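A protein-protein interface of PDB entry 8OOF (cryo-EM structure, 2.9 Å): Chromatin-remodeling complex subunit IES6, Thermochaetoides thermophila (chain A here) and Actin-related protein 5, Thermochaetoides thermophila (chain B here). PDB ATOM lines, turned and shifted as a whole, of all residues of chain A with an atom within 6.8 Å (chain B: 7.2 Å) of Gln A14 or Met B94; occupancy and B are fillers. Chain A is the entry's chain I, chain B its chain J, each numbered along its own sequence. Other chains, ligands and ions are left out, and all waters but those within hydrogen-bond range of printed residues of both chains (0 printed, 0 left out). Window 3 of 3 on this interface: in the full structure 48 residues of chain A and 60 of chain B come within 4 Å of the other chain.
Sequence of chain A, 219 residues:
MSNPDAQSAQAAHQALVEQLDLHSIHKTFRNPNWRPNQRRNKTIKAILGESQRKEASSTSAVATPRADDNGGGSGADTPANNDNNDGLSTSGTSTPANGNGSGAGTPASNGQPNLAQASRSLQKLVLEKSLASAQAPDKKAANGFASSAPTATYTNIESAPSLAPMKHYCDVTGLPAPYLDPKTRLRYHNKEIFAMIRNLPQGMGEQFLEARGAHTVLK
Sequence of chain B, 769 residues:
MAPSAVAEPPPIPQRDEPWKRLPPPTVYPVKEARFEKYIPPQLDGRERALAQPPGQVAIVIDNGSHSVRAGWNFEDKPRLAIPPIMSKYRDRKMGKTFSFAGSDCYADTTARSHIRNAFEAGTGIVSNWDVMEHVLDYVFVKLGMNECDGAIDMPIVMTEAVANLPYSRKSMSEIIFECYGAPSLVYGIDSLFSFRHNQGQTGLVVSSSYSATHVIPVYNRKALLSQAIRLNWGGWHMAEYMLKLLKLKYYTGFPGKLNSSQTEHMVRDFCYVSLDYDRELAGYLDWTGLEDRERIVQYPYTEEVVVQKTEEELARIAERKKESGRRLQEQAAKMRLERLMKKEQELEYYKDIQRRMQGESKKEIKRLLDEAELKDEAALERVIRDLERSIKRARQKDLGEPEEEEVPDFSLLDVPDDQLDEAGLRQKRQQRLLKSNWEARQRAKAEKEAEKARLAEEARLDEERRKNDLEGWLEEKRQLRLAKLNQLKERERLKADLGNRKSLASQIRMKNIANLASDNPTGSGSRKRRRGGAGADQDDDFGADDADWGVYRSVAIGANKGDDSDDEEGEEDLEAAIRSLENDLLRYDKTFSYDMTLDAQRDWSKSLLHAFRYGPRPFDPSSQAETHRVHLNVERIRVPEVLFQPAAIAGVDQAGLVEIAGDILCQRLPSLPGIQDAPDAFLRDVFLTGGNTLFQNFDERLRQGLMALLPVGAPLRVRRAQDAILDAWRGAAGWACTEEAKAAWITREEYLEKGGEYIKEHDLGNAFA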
ATOM      1  N   SER A   8     -19.893  14.934   2.373  1.00  0.00           N
ATOM      2  CA  SER A   8     -21.299  15.260   2.152  1.00  0.00           C
ATOM      3  C   SER A   8     -21.480  16.629   1.508  1.00  0.00           C
ATOM      4  O   SER A   8     -22.410  16.822   0.719  1.00  0.00           O
ATOM      5  CB  SER A   8     -22.062  15.196   3.476  1.00  0.00           C
ATOM      6  OG  SER A   8     -21.857  13.952   4.122  1.00  0.00           O
ATOM      7  N   ALA A   9     -20.608  17.588   1.832  1.00  0.00           N
ATOM      8  CA  ALA A   9     -20.705  18.912   1.225  1.00  0.00           C
ATOM      9  C   ALA A   9     -20.515  18.852  -0.285  1.00  0.00           C
ATOM     10  O   ALA A   9     -21.245  19.510  -1.036  1.00  0.00           O
ATOM     11  CB  ALA A   9     -19.681  19.853   1.858  1.00  0.00           C
ATOM     12  N   GLN A  10     -19.539  18.072  -0.753  1.00  0.00           N
ATOM     13  CA  GLN A  10     -19.366  17.896  -2.192  1.00  0.00           C
ATOM     14  C   GLN A  10     -20.529  17.121  -2.800  1.00  0.00           C
ATOM     15  O   GLN A  10     -20.990  17.444  -3.900  1.00  0.00           O
ATOM     16  CB  GLN A  10     -18.034  17.196  -2.472  1.00  0.00           C
ATOM     17  CG  GLN A  10     -17.703  16.999  -3.951  1.00  0.00           C
ATOM     18  CD  GLN A  10     -18.262  15.708  -4.526  1.00  0.00           C
ATOM     19  OE1 GLN A  10     -18.890  14.917  -3.821  1.00  0.00           O
ATOM     20  NE2 GLN A  10     -18.033  15.489  -5.815  1.00  0.00           N
ATOM     21  N   ALA A  11     -21.007  16.089  -2.103  1.00  0.00           N
ATOM     22  CA  ALA A  11     -22.158  15.326  -2.577  1.00  0.00           C
ATOM     23  C   ALA A  11     -23.413  16.189  -2.653  1.00  0.00           C
ATOM     24  O   ALA A  11     -24.153  16.144  -3.642  1.00  0.00           O
ATOM     25  CB  ALA A  11     -22.391  14.117  -1.671  1.00  0.00           C
ATOM     26  N   ALA A  12     -23.669  16.984  -1.611  1.00  0.00           N
ATOM     27  CA  ALA A  12     -24.802  17.903  -1.633  1.00  0.00           C
ATOM     28  C   ALA A  12     -24.688  18.926  -2.756  1.00  0.00           C
ATOM     29  O   ALA A  12     -25.677  19.222  -3.437  1.00  0.00           O
ATOM     30  CB  ALA A  12     -24.928  18.609  -0.283  1.00  0.00           C
ATOM     31  N   HIS A  13     -23.495  19.482  -2.964  1.00  0.00           N
ATOM     32  CA  HIS A  13     -23.294  20.417  -4.068  1.00  0.00           C
ATOM     33  C   HIS A  13     -23.543  19.753  -5.419  1.00  0.00           C
ATOM     34  O   HIS A  13     -24.201  20.329  -6.292  1.00  0.00           O
ATOM     35  CB  HIS A  13     -21.886  21.004  -4.009  1.00  0.00           C
ATOM     36  CG  HIS A  13     -21.639  22.078  -5.022  1.00  0.00           C
ATOM     37  ND1 HIS A  13     -21.066  21.825  -6.249  1.00  0.00           N
ATOM     38  CD2 HIS A  13     -21.896  23.407  -4.993  1.00  0.00           C
ATOM     39  CE1 HIS A  13     -20.975  22.954  -6.931  1.00  0.00           C
ATOM     40  NE2 HIS A  13     -21.473  23.928  -6.191  1.00  0.00           N
ATOM     41  N   GLN A  14     -23.019  18.543  -5.612  1.00  0.00           N
ATOM     42  CA  GLN A  14     -23.311  17.799  -6.835  1.00  0.00           C
ATOM     43  C   GLN A  14     -24.784  17.422  -6.946  1.00  0.00           C
ATOM     44  O   GLN A  14     -25.324  17.370  -8.058  1.00  0.00           O
ATOM     45  CB  GLN A  14     -22.444  16.542  -6.906  1.00  0.00           C
ATOM     46  CG  GLN A  14     -20.987  16.803  -7.248  1.00  0.00           C
ATOM     47  CD  GLN A  14     -20.797  17.357  -8.648  1.00  0.00           C
ATOM     48  OE1 GLN A  14     -21.707  17.315  -9.478  1.00  0.00           O
ATOM     49  NE2 GLN A  14     -19.608  17.882  -8.918  1.00  0.00           N
ATOM     50  N   ALA A  15     -25.444  17.144  -5.823  1.00  0.00           N
ATOM     51  CA  ALA A  15     -26.887  16.924  -5.847  1.00  0.00           C
ATOM     52  C   ALA A  15     -27.641  18.162  -6.320  1.00  0.00           C
ATOM     53  O   ALA A  15     -28.520  18.074  -7.185  1.00  0.00           O
ATOM     54  CB  ALA A  15     -27.371  16.500  -4.460  1.00  0.00           C
ATOM     55  N   LEU A  16     -27.305  19.328  -5.765  1.00  0.00           N
ATOM     56  CA  LEU A  16     -27.893  20.587  -6.223  1.00  0.00           C
ATOM     57  C   LEU A  16     -27.595  20.868  -7.692  1.00  0.00           C
ATOM     58  O   LEU A  16     -28.487  21.271  -8.447  1.00  0.00           O
ATOM     59  CB  LEU A  16     -27.391  21.740  -5.354  1.00  0.00           C
ATOM     60  CG  LEU A  16     -28.252  22.178  -4.167  1.00  0.00           C
ATOM     61  CD1 LEU A  16     -29.488  22.917  -4.650  1.00  0.00           C
ATOM     62  CD2 LEU A  16     -28.640  20.990  -3.297  1.00  0.00           C
ATOM     63  N   VAL A  17     -26.347  20.672  -8.116  1.00  0.00           N
ATOM     64  CA  VAL A  17     -25.991  20.909  -9.514  1.00  0.00           C
ATOM     65  C   VAL A  17     -26.809  20.031 -10.454  1.00  0.00           C
ATOM     66  O   VAL A  17     -27.311  20.500 -11.483  1.00  0.00           O
ATOM     67  CB  VAL A  17     -24.479  20.707  -9.717  1.00  0.00           C
ATOM     68  CG1 VAL A  17     -24.166  20.450 -11.179  1.00  0.00           C
ATOM     69  CG2 VAL A  17     -23.717  21.923  -9.221  1.00  0.00           C
ATOM     70  N   GLU A  18     -26.960  18.749 -10.125  1.00  0.00           N
ATOM     71  CA  GLU A  18     -27.812  17.878 -10.929  1.00  0.00           C
ATOM     72  C   GLU A  18     -29.284  18.259 -10.814  1.00  0.00           C
ATOM     73  O   GLU A  18     -30.014  18.245 -11.812  1.00  0.00           O
ATOM     74  CB  GLU A  18     -27.604  16.421 -10.516  1.00  0.00           C
ATOM     75  CG  GLU A  18     -28.471  15.437 -11.278  1.00  0.00           C
ATOM     76  CD  GLU A  18     -28.178  15.441 -12.765  1.00  0.00           C
ATOM     77  OE1 GLU A  18     -26.988  15.355 -13.136  1.00  0.00           O
ATOM     78  OE2 GLU A  18     -29.134  15.536 -13.561  1.00  0.00           O
ATOM     79  N   GLN A  19     -29.736  18.602  -9.608  1.00  0.00           N
ATOM     80  CA  GLN A  19     -31.128  18.998  -9.403  1.00  0.00           C
ATOM     81  C   GLN A  19     -31.485  20.262 -10.179  1.00  0.00           C
ATOM     82  O   GLN A  19     -32.599  20.385 -10.700  1.00  0.00           O
ATOM     83  CB  GLN A  19     -31.388  19.192  -7.911  1.00  0.00           C
ATOM     84  CG  GLN A  19     -32.772  19.694  -7.565  1.00  0.00           C
ATOM     85  CD  GLN A  19     -33.039  19.631  -6.077  1.00  0.00           C
ATOM     86  OE1 GLN A  19     -32.140  19.346  -5.288  1.00  0.00           O
ATOM     87  NE2 GLN A  19     -34.280  19.890  -5.686  1.00  0.00           N
ATOM     88  N   ARG B  90     -18.954  22.095 -18.933  1.00  0.00           N
ATOM     89  CA  ARG B  90     -18.706  20.727 -18.493  1.00  0.00           C
ATOM     90  C   ARG B  90     -17.876  20.733 -17.218  1.00  0.00           C
ATOM     91  O   ARG B  90     -16.856  21.424 -17.143  1.00  0.00           O
ATOM     92  CB  ARG B  90     -17.971  19.928 -19.571  1.00  0.00           C
ATOM     93  CG  ARG B  90     -18.852  19.395 -20.679  1.00  0.00           C
ATOM     94  CD  ARG B  90     -18.012  18.785 -21.789  1.00  0.00           C
ATOM     95  NE  ARG B  90     -17.361  19.796 -22.613  1.00  0.00           N
ATOM     96  CZ  ARG B  90     -17.964  20.490 -23.569  1.00  0.00           C
ATOM     97  NH1 ARG B  90     -19.259  20.360 -23.806  1.00  0.00           N
ATOM     98  NH2 ARG B  90     -17.254  21.350 -24.292  1.00  0.00           N
ATOM     99  N   ASP B  91     -18.301  19.955 -16.224  1.00  0.00           N
ATOM    100  CA  ASP B  91     -17.369  19.431 -15.228  1.00  0.00           C
ATOM    101  C   ASP B  91     -16.487  18.381 -15.889  1.00  0.00           C
ATOM    102  O   ASP B  91     -16.879  17.221 -16.023  1.00  0.00           O
ATOM    103  CB  ASP B  91     -18.121  18.844 -14.039  1.00  0.00           C
ATOM    104  CG  ASP B  91     -18.367  19.862 -12.945  1.00  0.00           C
ATOM    105  OD1 ASP B  91     -17.793  20.969 -13.019  1.00  0.00           O
ATOM    106  OD2 ASP B  91     -19.126  19.551 -12.003  1.00  0.00           O
ATOM    107  N   ARG B  92     -15.288  18.789 -16.314  1.00  0.00           N
ATOM    108  CA  ARG B  92     -14.512  17.956 -17.225  1.00  0.00           C
ATOM    109  C   ARG B  92     -14.065  16.656 -16.566  1.00  0.00           C
ATOM    110  O   ARG B  92     -13.862  15.651 -17.257  1.00  0.00           O
ATOM    111  CB  ARG B  92     -13.306  18.733 -17.749  1.00  0.00           C
ATOM    112  CG  ARG B  92     -12.852  18.293 -19.127  1.00  0.00           C
ATOM    113  CD  ARG B  92     -13.910  18.623 -20.169  1.00  0.00           C
ATOM    114  NE  ARG B  92     -13.418  18.454 -21.530  1.00  0.00           N
ATOM    115  CZ  ARG B  92     -12.835  19.412 -22.238  1.00  0.00           C
ATOM    116  NH1 ARG B  92     -12.654  20.625 -21.741  1.00  0.00           N
ATOM    117  NH2 ARG B  92     -12.425  19.147 -23.474  1.00  0.00           N
ATOM    118  N   LYS B  93     -13.907  16.655 -15.240  1.00  0.00           N
ATOM    119  CA  LYS B  93     -13.711  15.412 -14.504  1.00  0.00           C
ATOM    120  C   LYS B  93     -14.946  14.521 -14.513  1.00  0.00           C
ATOM    121  O   LYS B  93     -14.817  13.306 -14.324  1.00  0.00           O
ATOM    122  CB  LYS B  93     -13.304  15.718 -13.063  1.00  0.00           C
ATOM    123  CG  LYS B  93     -14.371  16.437 -12.255  1.00  0.00           C
ATOM    124  CD  LYS B  93     -13.875  16.757 -10.857  1.00  0.00           C
ATOM    125  CE  LYS B  93     -14.925  17.507 -10.057  1.00  0.00           C
ATOM    126  NZ  LYS B  93     -14.436  17.851  -8.694  1.00  0.00           N
ATOM    127  N   MET B  94     -16.132  15.089 -14.723  1.00  0.00           N
ATOM    128  CA  MET B  94     -17.368  14.320 -14.686  1.00  0.00           C
ATOM    129  C   MET B  94     -17.946  14.056 -16.070  1.00  0.00           C
ATOM    130  O   MET B  94     -18.773  13.149 -16.217  1.00  0.00           O
ATOM    131  CB  MET B  94     -18.408  15.046 -13.822  1.00  0.00           C
ATOM    132  CG  MET B  94     -19.509  14.154 -13.279  1.00  0.00           C
ATOM    133  SD  MET B  94     -20.597  15.035 -12.142  1.00  0.00           S
ATOM    134  CE  MET B  94     -21.578  13.683 -11.497  1.00  0.00           C
ATOM    135  N   GLY B  95     -17.526  14.815 -17.077  1.00  0.00           N
ATOM    136  CA  GLY B  95     -17.865  14.538 -18.459  1.00  0.00           C
ATOM    137  C   GLY B  95     -19.226  15.048 -18.887  1.00  0.00           C
ATOM    138  O   GLY B  95     -19.381  15.533 -20.011  1.00  0.00           O
ATOM    139  N   LYS B  96     -20.221  14.941 -18.010  1.00  0.00           N
ATOM    140  CA  LYS B  96     -21.546  15.453 -18.329  1.00  0.00           C
ATOM    141  C   LYS B  96     -21.528  16.974 -18.421  1.00  0.00           C
ATOM    142  O   LYS B  96     -20.872  17.656 -17.630  1.00  0.00           O
ATOM    143  CB  LYS B  96     -22.567  14.975 -17.297  1.00  0.00           C
ATOM    144  CG  LYS B  96     -22.189  15.214 -15.853  1.00  0.00           C
ATOM    145  CD  LYS B  96     -23.385  14.972 -14.949  1.00  0.00           C
ATOM    146  CE  LYS B  96     -23.979  13.591 -15.169  1.00  0.00           C
ATOM    147  NZ  LYS B  96     -25.071  13.296 -14.201  1.00  0.00           N
ATOM    148  N   THR B  97     -22.262  17.501 -19.396  1.00  0.00           N
ATOM    149  CA  THR B  97     -22.488  18.933 -19.510  1.00  0.00           C
ATOM    150  C   THR B  97     -23.596  19.381 -18.565  1.00  0.00           C
ATOM    151  O   THR B  97     -24.582  18.670 -18.355  1.00  0.00           O
ATOM    152  CB  THR B  97     -22.852  19.293 -20.953  1.00  0.00           C
ATOM    153  OG1 THR B  97     -21.794  18.881 -21.826  1.00  0.00           O
ATOM    154  CG2 THR B  97     -23.056  20.789 -21.108  1.00  0.00           C
ATOM    155  N   PHE B  98     -23.426  20.570 -17.991  1.00  0.00           N
ATOM    156  CA  PHE B  98     -24.459  21.214 -17.198  1.00  0.00           C
ATOM    157  C   PHE B  98     -24.866  22.526 -17.850  1.00  0.00           C
ATOM    158  O   PHE B  98     -24.068  23.176 -18.531  1.00  0.00           O
ATOM    159  CB  PHE B  98     -23.992  21.501 -15.770  1.00  0.00           C
ATOM    160  CG  PHE B  98     -23.646  20.280 -14.981  1.00  0.00           C
ATOM    161  CD1 PHE B  98     -24.610  19.335 -14.686  1.00  0.00           C
ATOM    162  CD2 PHE B  98     -22.362  20.090 -14.506  1.00  0.00           C
ATOM    163  CE1 PHE B  98     -24.295  18.214 -13.950  1.00  0.00           C
ATOM    164  CE2 PHE B  98     -22.041  18.973 -13.770  1.00  0.00           C
ATOM    165  CZ  PHE B  98     -23.009  18.035 -13.489  1.00  0.00           C
ATOM    166  N   ARG B 112     -19.627  28.267 -10.426  1.00  0.00           N
ATOM    167  CA  ARG B 112     -18.671  28.690 -11.443  1.00  0.00           C
ATOM    168  C   ARG B 112     -18.951  30.109 -11.924  1.00  0.00           C
ATOM    169  O   ARG B 112     -18.017  30.828 -12.301  1.00  0.00           O
ATOM    170  CB  ARG B 112     -18.692  27.721 -12.624  1.00  0.00           C
ATOM    171  CG  ARG B 112     -18.546  26.267 -12.227  1.00  0.00           C
ATOM    172  CD  ARG B 112     -17.298  26.037 -11.401  1.00  0.00           C
ATOM    173  NE  ARG B 112     -17.118  24.627 -11.081  1.00  0.00           N
ATOM    174  CZ  ARG B 112     -16.974  24.149  -9.853  1.00  0.00           C
ATOM    175  NH1 ARG B 112     -16.933  24.950  -8.801  1.00  0.00           N
ATOM    176  NH2 ARG B 112     -16.847  22.837  -9.678  1.00  0.00           N
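OE1 of Gln A14 sits close to SD of Met B94. The side-chain carboxylate (OE1) of Glu A18 lies within salt-bridge range of the side-chain amino group (NZ) of Lys B96 (3.0 Å).
NH2 of Arg B112 is in salt-bridge range of OD1 of Asp B91, 3.9 Å away.
NE2 of Gln A14 touches OD2 of Asp B91, 3.5 Å away. CG1 of Val A17 touches CZ of Phe B98, 3.5 Å away.
Of chain B, only Asp B91 (3.5 Å) and Met B94 (3.7 Å) come within 4 Å of Gln A14. Of chain A, only Gln A14 comes within 4 Å of Met B94. Printed residues of chain B within 4 Å of Val A17: Phe B98 (3.5 Å). Printed residues of chain B within 4 Å of Glu A18: Lys B96 (3.0 Å). Printed residues of chain A within 4 Å of Lys B96: Glu A18. Printed residues of chain A within 4 Å of Asp B91: Gln A14. Lys B93 touches none of the printed residues of chain A. The nearest residue of chain B that does not touch Gln A14 is Phe B98 (4.3 Å). The nearest residue of chain A that does not touch Met B94 is Glu A18 (5.9 Å). The nearest printed residue of chain A that does not touch Phe B98 is Glu A18 (4.01 Å).
Of the 10 printed residues of chain B, 4 touch a printed residue of chain A. Hydrophobic or aromatic side chains of chain A within 4 Å of the printed part of chain B: Val A17. Among the printed residues, Asp or Glu carboxylates within 4 Å of a Lys or Arg side-chain nitrogen of the other chain: Glu A18 with Lys B96 (3.0 Å).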
